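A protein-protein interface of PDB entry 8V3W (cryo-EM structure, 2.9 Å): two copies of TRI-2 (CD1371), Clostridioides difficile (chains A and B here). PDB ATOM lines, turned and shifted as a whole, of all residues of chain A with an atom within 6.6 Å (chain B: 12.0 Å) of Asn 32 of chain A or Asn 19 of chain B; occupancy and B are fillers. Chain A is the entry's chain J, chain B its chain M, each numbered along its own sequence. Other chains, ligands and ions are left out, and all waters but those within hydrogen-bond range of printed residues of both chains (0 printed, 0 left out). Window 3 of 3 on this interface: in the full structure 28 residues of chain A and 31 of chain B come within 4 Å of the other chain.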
ATOM      1  N   LYS A  11     -16.763  21.716  21.697  1.00  0.00           N
ATOM      2  CA  LYS A  11     -17.599  20.834  22.503  1.00  0.00           C
ATOM      3  C   LYS A  11     -17.614  21.274  23.961  1.00  0.00           C
ATOM      4  O   LYS A  11     -18.677  21.326  24.595  1.00  0.00           O
ATOM      5  CB  LYS A  11     -17.107  19.394  22.371  1.00  0.00           C
ATOM      6  CG  LYS A  11     -17.903  18.376  23.162  1.00  0.00           C
ATOM      7  CD  LYS A  11     -17.360  16.976  22.928  1.00  0.00           C
ATOM      8  CE  LYS A  11     -18.200  15.930  23.632  1.00  0.00           C
ATOM      9  NZ  LYS A  11     -18.531  16.349  25.020  1.00  0.00           N
ATOM     10  N   GLY A  25     -21.273  14.358  31.001  1.00  0.00           N
ATOM     11  CA  GLY A  25     -20.158  13.438  31.079  1.00  0.00           C
ATOM     12  C   GLY A  25     -20.367  12.262  30.154  1.00  0.00           C
ATOM     13  O   GLY A  25     -21.316  12.227  29.369  1.00  0.00           O
ATOM     14  N   GLU A  26     -19.463  11.292  30.259  1.00  0.00           N
ATOM     15  CA  GLU A  26     -19.518  10.125  29.390  1.00  0.00           C
ATOM     16  C   GLU A  26     -20.833   9.383  29.583  1.00  0.00           C
ATOM     17  O   GLU A  26     -21.270   9.152  30.713  1.00  0.00           O
ATOM     18  CB  GLU A  26     -18.343   9.189  29.678  1.00  0.00           C
ATOM     19  CG  GLU A  26     -16.999   9.656  29.129  1.00  0.00           C
ATOM     20  CD  GLU A  26     -16.753   9.210  27.696  1.00  0.00           C
ATOM     21  OE1 GLU A  26     -17.715   9.185  26.899  1.00  0.00           O
ATOM     22  OE2 GLU A  26     -15.595   8.875  27.368  1.00  0.00           O
ATOM     23  N   GLY A  27     -21.462   9.012  28.473  1.00  0.00           N
ATOM     24  CA  GLY A  27     -22.723   8.296  28.539  1.00  0.00           C
ATOM     25  C   GLY A  27     -23.867   9.104  29.111  1.00  0.00           C
ATOM     26  O   GLY A  27     -24.691   8.563  29.857  1.00  0.00           O
ATOM     27  N   SER A  28     -23.937  10.389  28.783  1.00  0.00           N
ATOM     28  CA  SER A  28     -25.012  11.262  29.222  1.00  0.00           C
ATOM     29  C   SER A  28     -25.822  11.726  28.018  1.00  0.00           C
ATOM     30  O   SER A  28     -25.311  11.802  26.897  1.00  0.00           O
ATOM     31  CB  SER A  28     -24.464  12.472  29.980  1.00  0.00           C
ATOM     32  OG  SER A  28     -25.486  13.124  30.709  1.00  0.00           O
ATOM     33  N   PHE A  29     -27.099  12.024  28.263  1.00  0.00           N
ATOM     34  CA  PHE A  29     -27.985  12.462  27.186  1.00  0.00           C
ATOM     35  C   PHE A  29     -27.451  13.728  26.525  1.00  0.00           C
ATOM     36  O   PHE A  29     -27.234  13.774  25.303  1.00  0.00           O
ATOM     37  CB  PHE A  29     -29.388  12.688  27.759  1.00  0.00           C
ATOM     38  CG  PHE A  29     -30.415  13.112  26.746  1.00  0.00           C
ATOM     39  CD1 PHE A  29     -30.579  14.445  26.414  1.00  0.00           C
ATOM     40  CD2 PHE A  29     -31.242  12.176  26.151  1.00  0.00           C
ATOM     41  CE1 PHE A  29     -31.529  14.832  25.492  1.00  0.00           C
ATOM     42  CE2 PHE A  29     -32.193  12.556  25.232  1.00  0.00           C
ATOM     43  CZ  PHE A  29     -32.336  13.886  24.901  1.00  0.00           C
ATOM     44  N   LEU A  30     -27.192  14.756  27.334  1.00  0.00           N
ATOM     45  CA  LEU A  30     -26.743  16.033  26.796  1.00  0.00           C
ATOM     46  C   LEU A  30     -25.376  15.911  26.141  1.00  0.00           C
ATOM     47  O   LEU A  30     -25.139  16.497  25.081  1.00  0.00           O
ATOM     48  CB  LEU A  30     -26.711  17.084  27.900  1.00  0.00           C
ATOM     49  CG  LEU A  30     -26.971  18.507  27.418  1.00  0.00           C
ATOM     50  CD1 LEU A  30     -28.277  18.589  26.650  1.00  0.00           C
ATOM     51  CD2 LEU A  30     -26.975  19.461  28.584  1.00  0.00           C
ATOM     52  N   ASN A  31     -24.463  15.158  26.757  1.00  0.00           N
ATOM     53  CA  ASN A  31     -23.124  15.013  26.195  1.00  0.00           C
ATOM     54  C   ASN A  31     -23.174  14.361  24.819  1.00  0.00           C
ATOM     55  O   ASN A  31     -22.521  14.820  23.875  1.00  0.00           O
ATOM     56  CB  ASN A  31     -22.248  14.207  27.152  1.00  0.00           C
ATOM     57  CG  ASN A  31     -20.848  13.970  26.616  1.00  0.00           C
ATOM     58  OD1 ASN A  31     -19.903  14.656  26.999  1.00  0.00           O
ATOM     59  ND2 ASN A  31     -20.702  12.971  25.753  1.00  0.00           N
ATOM     60  N   ASN A  32     -23.959  13.292  24.687  1.00  0.00           N
ATOM     61  CA  ASN A  32     -24.047  12.598  23.409  1.00  0.00           C
ATOM     62  C   ASN A  32     -24.682  13.479  22.340  1.00  0.00           C
ATOM     63  O   ASN A  32     -24.173  13.561  21.213  1.00  0.00           O
ATOM     64  CB  ASN A  32     -24.832  11.303  23.579  1.00  0.00           C
ATOM     65  CG  ASN A  32     -24.172  10.352  24.547  1.00  0.00           C
ATOM     66  OD1 ASN A  32     -22.984  10.473  24.837  1.00  0.00           O
ATOM     67  ND2 ASN A  32     -24.944   9.404  25.066  1.00  0.00           N
ATOM     68  N   MET A  33     -25.783  14.156  22.678  1.00  0.00           N
ATOM     69  CA  MET A  33     -26.418  15.035  21.702  1.00  0.00           C
ATOM     70  C   MET A  33     -25.476  16.159  21.276  1.00  0.00           C
ATOM     71  O   MET A  33     -25.366  16.480  20.081  1.00  0.00           O
ATOM     72  CB  MET A  33     -27.714  15.594  22.286  1.00  0.00           C
ATOM     73  CG  MET A  33     -28.066  16.999  21.855  1.00  0.00           C
ATOM     74  SD  MET A  33     -29.661  17.509  22.520  1.00  0.00           S
ATOM     75  CE  MET A  33     -29.623  19.263  22.178  1.00  0.00           C
ATOM     76  N   VAL A  34     -24.770  16.749  22.240  1.00  0.00           N
ATOM     77  CA  VAL A  34     -23.871  17.858  21.950  1.00  0.00           C
ATOM     78  C   VAL A  34     -22.730  17.407  21.049  1.00  0.00           C
ATOM     79  O   VAL A  34     -22.364  18.107  20.098  1.00  0.00           O
ATOM     80  CB  VAL A  34     -23.359  18.471  23.264  1.00  0.00           C
ATOM     81  CG1 VAL A  34     -22.093  19.252  23.032  1.00  0.00           C
ATOM     82  CG2 VAL A  34     -24.425  19.365  23.868  1.00  0.00           C
ATOM     83  N   SER A  35     -22.148  16.239  21.327  1.00  0.00           N
ATOM     84  CA  SER A  35     -21.074  15.744  20.471  1.00  0.00           C
ATOM     85  C   SER A  35     -21.575  15.464  19.057  1.00  0.00           C
ATOM     86  O   SER A  35     -20.906  15.806  18.067  1.00  0.00           O
ATOM     87  CB  SER A  35     -20.454  14.490  21.085  1.00  0.00           C
ATOM     88  OG  SER A  35     -21.414  13.462  21.225  1.00  0.00           O
ATOM     89  N   GLY A  36     -22.758  14.853  18.943  1.00  0.00           N
ATOM     90  CA  GLY A  36     -23.308  14.566  17.629  1.00  0.00           C
ATOM     91  C   GLY A  36     -23.549  15.816  16.806  1.00  0.00           C
ATOM     92  O   GLY A  36     -23.383  15.808  15.584  1.00  0.00           O
ATOM     93  N   ASN A  37     -23.955  16.908  17.458  1.00  0.00           N
ATOM     94  CA  ASN A  37     -24.111  18.164  16.726  1.00  0.00           C
ATOM     95  C   ASN A  37     -22.765  18.810  16.410  1.00  0.00           C
ATOM     96  O   ASN A  37     -22.566  19.359  15.316  1.00  0.00           O
ATOM     97  CB  ASN A  37     -24.990  19.132  17.514  1.00  0.00           C
ATOM     98  CG  ASN A  37     -26.313  19.394  16.837  1.00  0.00           C
ATOM     99  OD1 ASN A  37     -26.490  19.079  15.662  1.00  0.00           O
ATOM    100  ND2 ASN A  37     -27.249  19.982  17.567  1.00  0.00           N
ATOM    101  N   LYS B  11     -29.532  16.870   8.670  1.00  0.00           N
ATOM    102  CA  LYS B  11     -30.308  16.376   9.802  1.00  0.00           C
ATOM    103  C   LYS B  11     -30.210  14.863   9.923  1.00  0.00           C
ATOM    104  O   LYS B  11     -30.044  14.330  11.026  1.00  0.00           O
ATOM    105  CB  LYS B  11     -31.763  16.802   9.649  1.00  0.00           C
ATOM    106  CG  LYS B  11     -32.576  16.771  10.918  1.00  0.00           C
ATOM    107  CD  LYS B  11     -34.044  16.748  10.575  1.00  0.00           C
ATOM    108  CE  LYS B  11     -34.867  17.458  11.611  1.00  0.00           C
ATOM    109  NZ  LYS B  11     -36.239  17.748  11.116  1.00  0.00           N
ATOM    110  N   ASN B  12     -30.313  14.153   8.798  1.00  0.00           N
ATOM    111  CA  ASN B  12     -30.245  12.698   8.829  1.00  0.00           C
ATOM    112  C   ASN B  12     -28.891  12.223   9.336  1.00  0.00           C
ATOM    113  O   ASN B  12     -28.815  11.321  10.179  1.00  0.00           O
ATOM    114  CB  ASN B  12     -30.534  12.144   7.435  1.00  0.00           C
ATOM    115  CG  ASN B  12     -30.716  10.644   7.424  1.00  0.00           C
ATOM    116  OD1 ASN B  12     -29.850   9.892   7.867  1.00  0.00           O
ATOM    117  ND2 ASN B  12     -31.856  10.197   6.917  1.00  0.00           N
ATOM    118  N   ARG B  13     -27.809  12.832   8.845  1.00  0.00           N
ATOM    119  CA  ARG B  13     -26.479  12.448   9.304  1.00  0.00           C
ATOM    120  C   ARG B  13     -26.299  12.745  10.787  1.00  0.00           C
ATOM    121  O   ARG B  13     -25.757  11.920  11.534  1.00  0.00           O
ATOM    122  CB  ARG B  13     -25.416  13.166   8.476  1.00  0.00           C
ATOM    123  CG  ARG B  13     -23.993  12.833   8.863  1.00  0.00           C
ATOM    124  CD  ARG B  13     -23.029  13.865   8.314  1.00  0.00           C
ATOM    125  NE  ARG B  13     -23.128  13.983   6.865  1.00  0.00           N
ATOM    126  CZ  ARG B  13     -23.430  15.102   6.225  1.00  0.00           C
ATOM    127  NH1 ARG B  13     -23.662  16.229   6.877  1.00  0.00           N
ATOM    128  NH2 ARG B  13     -23.505  15.092   4.898  1.00  0.00           N
ATOM    129  N   THR B  14     -26.758  13.917  11.236  1.00  0.00           N
ATOM    130  CA  THR B  14     -26.618  14.274  12.643  1.00  0.00           C
ATOM    131  C   THR B  14     -27.372  13.304  13.536  1.00  0.00           C
ATOM    132  O   THR B  14     -26.859  12.883  14.578  1.00  0.00           O
ATOM    133  CB  THR B  14     -27.113  15.697  12.877  1.00  0.00           C
ATOM    134  OG1 THR B  14     -26.407  16.598  12.015  1.00  0.00           O
ATOM    135  CG2 THR B  14     -26.894  16.102  14.319  1.00  0.00           C
ATOM    136  N   LEU B  15     -28.594  12.938  13.148  1.00  0.00           N
ATOM    137  CA  LEU B  15     -29.358  11.982  13.939  1.00  0.00           C
ATOM    138  C   LEU B  15     -28.689  10.615  13.949  1.00  0.00           C
ATOM    139  O   LEU B  15     -28.673   9.936  14.981  1.00  0.00           O
ATOM    140  CB  LEU B  15     -30.784  11.880  13.406  1.00  0.00           C
ATOM    141  CG  LEU B  15     -31.729  12.998  13.840  1.00  0.00           C
ATOM    142  CD1 LEU B  15     -33.062  12.854  13.142  1.00  0.00           C
ATOM    143  CD2 LEU B  15     -31.907  12.994  15.348  1.00  0.00           C
ATOM    144  N   GLU B  16     -28.136  10.190  12.810  1.00  0.00           N
ATOM    145  CA  GLU B  16     -27.445   8.907  12.775  1.00  0.00           C
ATOM    146  C   GLU B  16     -26.211   8.905  13.667  1.00  0.00           C
ATOM    147  O   GLU B  16     -25.862   7.865  14.232  1.00  0.00           O
ATOM    148  CB  GLU B  16     -27.056   8.556  11.341  1.00  0.00           C
ATOM    149  CG  GLU B  16     -26.767   7.082  11.128  1.00  0.00           C
ATOM    150  CD  GLU B  16     -28.024   6.272  10.889  1.00  0.00           C
ATOM    151  OE1 GLU B  16     -29.125   6.861  10.907  1.00  0.00           O
ATOM    152  OE2 GLU B  16     -27.912   5.046  10.687  1.00  0.00           O
ATOM    153  N   ASN B  17     -25.537  10.048  13.800  1.00  0.00           N
ATOM    154  CA  ASN B  17     -24.339  10.090  14.631  1.00  0.00           C
ATOM    155  C   ASN B  17     -24.662   9.964  16.114  1.00  0.00           C
ATOM    156  O   ASN B  17     -23.850   9.428  16.876  1.00  0.00           O
ATOM    157  CB  ASN B  17     -23.560  11.375  14.365  1.00  0.00           C
ATOM    158  CG  ASN B  17     -22.912  11.389  12.997  1.00  0.00           C
ATOM    159  OD1 ASN B  17     -23.036  10.437  12.227  1.00  0.00           O
ATOM    160  ND2 ASN B  17     -22.210  12.471  12.688  1.00  0.00           N
ATOM    161  N   ILE B  18     -25.825  10.447  16.548  1.00  0.00           N
ATOM    162  CA  ILE B  18     -26.167  10.422  17.967  1.00  0.00           C
ATOM    163  C   ILE B  18     -26.468   8.994  18.398  1.00  0.00           C
ATOM    164  O   ILE B  18     -27.279   8.298  17.774  1.00  0.00           O
ATOM    165  CB  ILE B  18     -27.360  11.345  18.250  1.00  0.00           C
ATOM    166  CG1 ILE B  18     -27.067  12.762  17.759  1.00  0.00           C
ATOM    167  CG2 ILE B  18     -27.671  11.365  19.732  1.00  0.00           C
ATOM    168  CD1 ILE B  18     -28.157  13.755  18.084  1.00  0.00           C
ATOM    169  N   ASN B  19     -25.821   8.550  19.473  1.00  0.00           N
ATOM    170  CA  ASN B  19     -25.988   7.196  19.998  1.00  0.00           C
ATOM    171  C   ASN B  19     -26.860   7.264  21.249  1.00  0.00           C
ATOM    172  O   ASN B  19     -26.369   7.263  22.377  1.00  0.00           O
ATOM    173  CB  ASN B  19     -24.619   6.559  20.289  1.00  0.00           C
ATOM    174  CG  ASN B  19     -24.712   5.073  20.590  1.00  0.00           C
ATOM    175  OD1 ASN B  19     -25.518   4.641  21.415  1.00  0.00           O
ATOM    176  ND2 ASN B  19     -23.882   4.283  19.919  1.00  0.00           N
ATOM    177  N   LEU B  20     -28.175   7.300  21.036  1.00  0.00           N
ATOM    178  CA  LEU B  20     -29.163   7.241  22.105  1.00  0.00           C
ATOM    179  C   LEU B  20     -30.156   6.128  21.814  1.00  0.00           C
ATOM    180  O   LEU B  20     -30.339   5.710  20.668  1.00  0.00           O
ATOM    181  CB  LEU B  20     -29.931   8.558  22.281  1.00  0.00           C
ATOM    182  CG  LEU B  20     -29.428   9.654  23.220  1.00  0.00           C
ATOM    183  CD1 LEU B  20     -29.730   9.275  24.658  1.00  0.00           C
ATOM    184  CD2 LEU B  20     -27.963   9.915  23.043  1.00  0.00           C
ATOM    185  N   ASP B  21     -30.804   5.654  22.876  1.00  0.00           N
ATOM    186  CA  ASP B  21     -31.771   4.573  22.757  1.00  0.00           C
ATOM    187  C   ASP B  21     -33.163   5.068  22.378  1.00  0.00           C
ATOM    188  O   ASP B  21     -33.968   4.284  21.869  1.00  0.00           O
ATOM    189  CB  ASP B  21     -31.828   3.798  24.074  1.00  0.00           C
ATOM    190  CG  ASP B  21     -32.775   2.616  24.024  1.00  0.00           C
ATOM    191  OD1 ASP B  21     -32.961   2.040  22.934  1.00  0.00           O
ATOM    192  OD2 ASP B  21     -33.332   2.260  25.082  1.00  0.00           O
ATOM    193  N   ILE B  22     -33.457   6.348  22.599  1.00  0.00           N
ATOM    194  CA  ILE B  22     -34.805   6.878  22.421  1.00  0.00           C
ATOM    195  C   ILE B  22     -35.181   6.942  20.947  1.00  0.00           C
ATOM    196  O   ILE B  22     -34.329   6.797  20.065  1.00  0.00           O
ATOM    197  CB  ILE B  22     -34.939   8.262  23.074  1.00  0.00           C
ATOM    198  CG1 ILE B  22     -34.115   9.289  22.303  1.00  0.00           C
ATOM    199  CG2 ILE B  22     -34.502   8.205  24.524  1.00  0.00           C
ATOM    200  CD1 ILE B  22     -34.061  10.630  22.972  1.00  0.00           C
ATOM    201  N   TYR B  23     -36.466   7.164  20.680  1.00  0.00           N
ATOM    202  CA  TYR B  23     -36.991   7.170  19.322  1.00  0.00           C
ATOM    203  C   TYR B  23     -36.667   8.489  18.637  1.00  0.00           C
ATOM    204  O   TYR B  23     -36.922   9.565  19.186  1.00  0.00           O
ATOM    205  CB  TYR B  23     -38.501   6.930  19.356  1.00  0.00           C
ATOM    206  CG  TYR B  23     -39.270   7.387  18.134  1.00  0.00           C
ATOM    207  CD1 TYR B  23     -39.377   6.575  17.018  1.00  0.00           C
ATOM    208  CD2 TYR B  23     -39.921   8.612  18.116  1.00  0.00           C
ATOM    209  CE1 TYR B  23     -40.088   6.975  15.910  1.00  0.00           C
ATOM    210  CE2 TYR B  23     -40.635   9.020  17.010  1.00  0.00           C
ATOM    211  CZ  TYR B  23     -40.714   8.198  15.910  1.00  0.00           C
ATOM    212  OH  TYR B  23     -41.423   8.599  14.805  1.00  0.00           O
ATOM    213  N   LYS B  24     -36.100   8.405  17.438  1.00  0.00           N
ATOM    214  CA  LYS B  24     -35.700   9.573  16.661  1.00  0.00           C
ATOM    215  C   LYS B  24     -36.605   9.663  15.442  1.00  0.00           C
ATOM    216  O   LYS B  24     -36.453   8.892  14.491  1.00  0.00           O
ATOM    217  CB  LYS B  24     -34.235   9.478  16.244  1.00  0.00           C
ATOM    218  CG  LYS B  24     -33.285   9.138  17.373  1.00  0.00           C
ATOM    219  CD  LYS B  24     -31.851   9.413  16.974  1.00  0.00           C
ATOM    220  CE  LYS B  24     -30.878   8.603  17.802  1.00  0.00           C
ATOM    221  NZ  LYS B  24     -30.402   7.409  17.058  1.00  0.00           N
ATOM    222  N   PHE B  29     -38.565  14.726  20.968  1.00  0.00           N
ATOM    223  CA  PHE B  29     -37.795  15.730  21.693  1.00  0.00           C
ATOM    224  C   PHE B  29     -36.412  15.912  21.081  1.00  0.00           C
ATOM    225  O   PHE B  29     -35.981  17.042  20.821  1.00  0.00           O
ATOM    226  CB  PHE B  29     -37.683  15.338  23.166  1.00  0.00           C
ATOM    227  CG  PHE B  29     -36.830  16.265  23.981  1.00  0.00           C
ATOM    228  CD1 PHE B  29     -37.369  17.408  24.541  1.00  0.00           C
ATOM    229  CD2 PHE B  29     -35.492  15.993  24.193  1.00  0.00           C
ATOM    230  CE1 PHE B  29     -36.588  18.260  25.295  1.00  0.00           C
ATOM    231  CE2 PHE B  29     -34.709  16.844  24.942  1.00  0.00           C
ATOM    232  CZ  PHE B  29     -35.258  17.979  25.493  1.00  0.00           C
ATOM    233  N   LEU B  30     -35.696  14.810  20.849  1.00  0.00           N
ATOM    234  CA  LEU B  30     -34.346  14.905  20.303  1.00  0.00           C
ATOM    235  C   LEU B  30     -34.358  15.511  18.907  1.00  0.00           C
ATOM    236  O   LEU B  30     -33.509  16.346  18.573  1.00  0.00           O
ATOM    237  CB  LEU B  30     -33.695  13.524  20.286  1.00  0.00           C
ATOM    238  CG  LEU B  30     -32.250  13.447  19.801  1.00  0.00           C
ATOM    239  CD1 LEU B  30     -31.316  14.067  20.819  1.00  0.00           C
ATOM    240  CD2 LEU B  30     -31.867  12.007  19.532  1.00  0.00           C
ATOM    241  N   ASN B  31     -35.321  15.102  18.079  1.00  0.00           N
ATOM    242  CA  ASN B  31     -35.459  15.681  16.750  1.00  0.00           C
ATOM    243  C   ASN B  31     -35.744  17.175  16.827  1.00  0.00           C
ATOM    244  O   ASN B  31     -35.170  17.963  16.069  1.00  0.00           O
ATOM    245  CB  ASN B  31     -36.562  14.942  15.992  1.00  0.00           C
ATOM    246  CG  ASN B  31     -36.600  15.280  14.520  1.00  0.00           C
ATOM    247  OD1 ASN B  31     -36.357  16.412  14.122  1.00  0.00           O
ATOM    248  ND2 ASN B  31     -36.900  14.287  13.699  1.00  0.00           N
ATOM    249  N   MET B  33     -34.916  19.242  19.242  1.00  0.00           N
ATOM    250  CA  MET B  33     -33.727  19.948  19.708  1.00  0.00           C
ATOM    251  C   MET B  33     -32.691  20.077  18.601  1.00  0.00           C
ATOM    252  O   MET B  33     -32.121  21.153  18.400  1.00  0.00           O
ATOM    253  CB  MET B  33     -33.119  19.226  20.908  1.00  0.00           C
ATOM    254  CG  MET B  33     -34.012  19.183  22.122  1.00  0.00           C
ATOM    255  SD  MET B  33     -33.981  20.703  23.073  1.00  0.00           S
ATOM    256  CE  MET B  33     -35.560  21.385  22.590  1.00  0.00           C
ATOM    257  N   VAL B  34     -32.434  18.989  17.875  1.00  0.00           N
ATOM    258  CA  VAL B  34     -31.408  19.014  16.840  1.00  0.00           C
ATOM    259  C   VAL B  34     -31.815  19.931  15.693  1.00  0.00           C
ATOM    260  O   VAL B  34     -31.007  20.725  15.202  1.00  0.00           O
ATOM    261  CB  VAL B  34     -31.115  17.584  16.358  1.00  0.00           C
ATOM    262  CG1 VAL B  34     -30.494  17.599  14.986  1.00  0.00           C
ATOM    263  CG2 VAL B  34     -30.189  16.898  17.336  1.00  0.00           C
ATOM    264  N   ASN B  37     -30.853  24.431  14.076  1.00  0.00           N
ATOM    265  CA  ASN B  37     -29.524  24.903  13.724  1.00  0.00           C
ATOM    266  C   ASN B  37     -28.942  24.184  12.516  1.00  0.00           C
ATOM    267  O   ASN B  37     -28.042  24.729  11.869  1.00  0.00           O
ATOM    268  CB  ASN B  37     -28.571  24.769  14.916  1.00  0.00           C
ATOM    269  CG  ASN B  37     -28.119  23.351  15.147  1.00  0.00           C
ATOM    270  OD1 ASN B  37     -28.868  22.404  14.928  1.00  0.00           O
ATOM    271  ND2 ASN B  37     -26.879  23.194  15.590  1.00  0.00           N
ATOM    272  N   ASN B  38     -29.430  22.984  12.195  1.00  0.00           N
ATOM    273  CA  ASN B  38     -29.057  22.346  10.938  1.00  0.00           C
ATOM    274  C   ASN B  38     -29.620  23.110   9.747  1.00  0.00           C
ATOM    275  O   ASN B  38     -28.978  23.193   8.692  1.00  0.00           O
ATOM    276  CB  ASN B  38     -29.535  20.898  10.925  1.00  0.00           C
ATOM    277  CG  ASN B  38     -28.925  20.078  12.038  1.00  0.00           C
ATOM    278  OD1 ASN B  38     -28.147  20.585  12.843  1.00  0.00           O
ATOM    279  ND2 ASN B  38     -29.271  18.800  12.086  1.00  0.00           N
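The side-chain amide oxygen of Asn 37 of chain B sits close to the side-chain amide oxygen of Asn 38 of chain B (2.9 Å).
ND2 of Asn 32 of chain A lies close to O of Ser 28 of chain A (3.0 Å).
The backbone carbonyl oxygen (O) of Asn 32 of chain A is in hydrogen-bond range of the side-chain hydroxyl (OG) of Ser 35 of chain A (2.8 Å).
OD1 of Asn 37 of chain B sits close to O of Val 34 of chain B, at 2.7 Å.
Phe 29 of chain A touches Leu 20 of chain B (CD2 to CD1, 3.6 Å).
Phe 29 of chain A touches Ile 22 of chain B.
Phe 29 of chain A touches Phe 29 of chain B (CZ to CE2, 3.8 Å).
Asn 32 of chain A touches Asn 19 of chain B.
Leu 20 of chain B touches Asn 32 of chain A (CD2 to CB, 3.5 Å).
Met 33 of chain A touches Met 33 of chain B (CE to CB, 3.7 Å).
O of Gly 36 of chain A touches CG2 of Thr 14 of chain B (3.7 Å).
OD1 of Asn 37 of chain A touches CG2 of Thr 14 of chain B, 3.3 Å away.
Asn 37 of chain A touches Asn 37 of chain B.
Asn 38 of chain B touches Asn 37 of chain A (OD1 to OD1, 3.6 Å).
No residue of chain B comes within 4 Å of Gly 25 of chain A.
No residue of chain B comes within 4 Å of Gly 27 of chain A.
No residue of chain B comes within 4 Å of Ser 28 of chain A.
Printed residues of chain B within 4 Å of Phe 29 of chain A: Leu 20, Ile 22 and Phe 29.
No residue of chain B comes within 4 Å of Leu 30 of chain A.
No residue of chain B comes within 4 Å of Asn 31 of chain A.
Asn 32 of chain A touches two residues of chain B.
Of chain B, only Met 33 (3.7 Å) comes within 4 Å of Met 33 of chain A.
No residue of chain B comes within 4 Å of Ser 35 of chain A.
Lys 11 of chain B touches none of the printed residues of chain A.
Asn 19 of chain B touches one residue of chain A.
Printed residues of chain A within 4 Å of Leu 20 of chain B: Phe 29 and Asn 32.
Of the printed residues of chain A, Ile 22 of chain B touches Phe 29 (3.5 Å).
Printed residues of chain A within 4 Å of Phe 29 of chain B: Phe 29 (3.8 Å).
Printed residues of chain A within 4 Å of Met 33 of chain B: Met 33.
Val 34 of chain B touches none of the printed residues of chain A.
The nearest residue of chain A that does not touch Asn 19 of chain B is Met 33 of chain A (6.5 Å).
The nearest printed residue of chain A that does not touch Leu 20 of chain B is Met 33 of chain A (4.8 Å).
Of the 14 printed residues of chain A, 5 touch a printed residue of chain B.
Hydrophobic or aromatic side chains of chain A that line the printed part of chain B: Phe 29 and Met 33.
Printed residues of chain B that touch a printed residue of chain A: Thr 14, Asn 19, Leu 20, Ile 22, Phe 29, Met 33, Asn 37 and Asn 38.
Hydrophobic or aromatic side chains of chain B within 4 Å of the printed part of chain A: Leu 20, Ile 22, Phe 29 and Met 33.
Among the printed residues, no Asp or Glu carboxylate lies within 4 Å of a Lys or Arg side-chain nitrogen of the other chain.
Phe 29 of chain B touches its own counterpart, Phe 29 of chain A.
Met 33 of chain A touches its own counterpart, Met 33 of chain B.
Asn 37 of chain B touches its own counterpart, Asn 37 of chain A.
Positions printed for both chains: 11, 29, 30, 31, 33, 34 and 37.
Of the 10 pairs that touch across the chains among the printed residues, 3 have their exchanged pair printed and touching as well.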
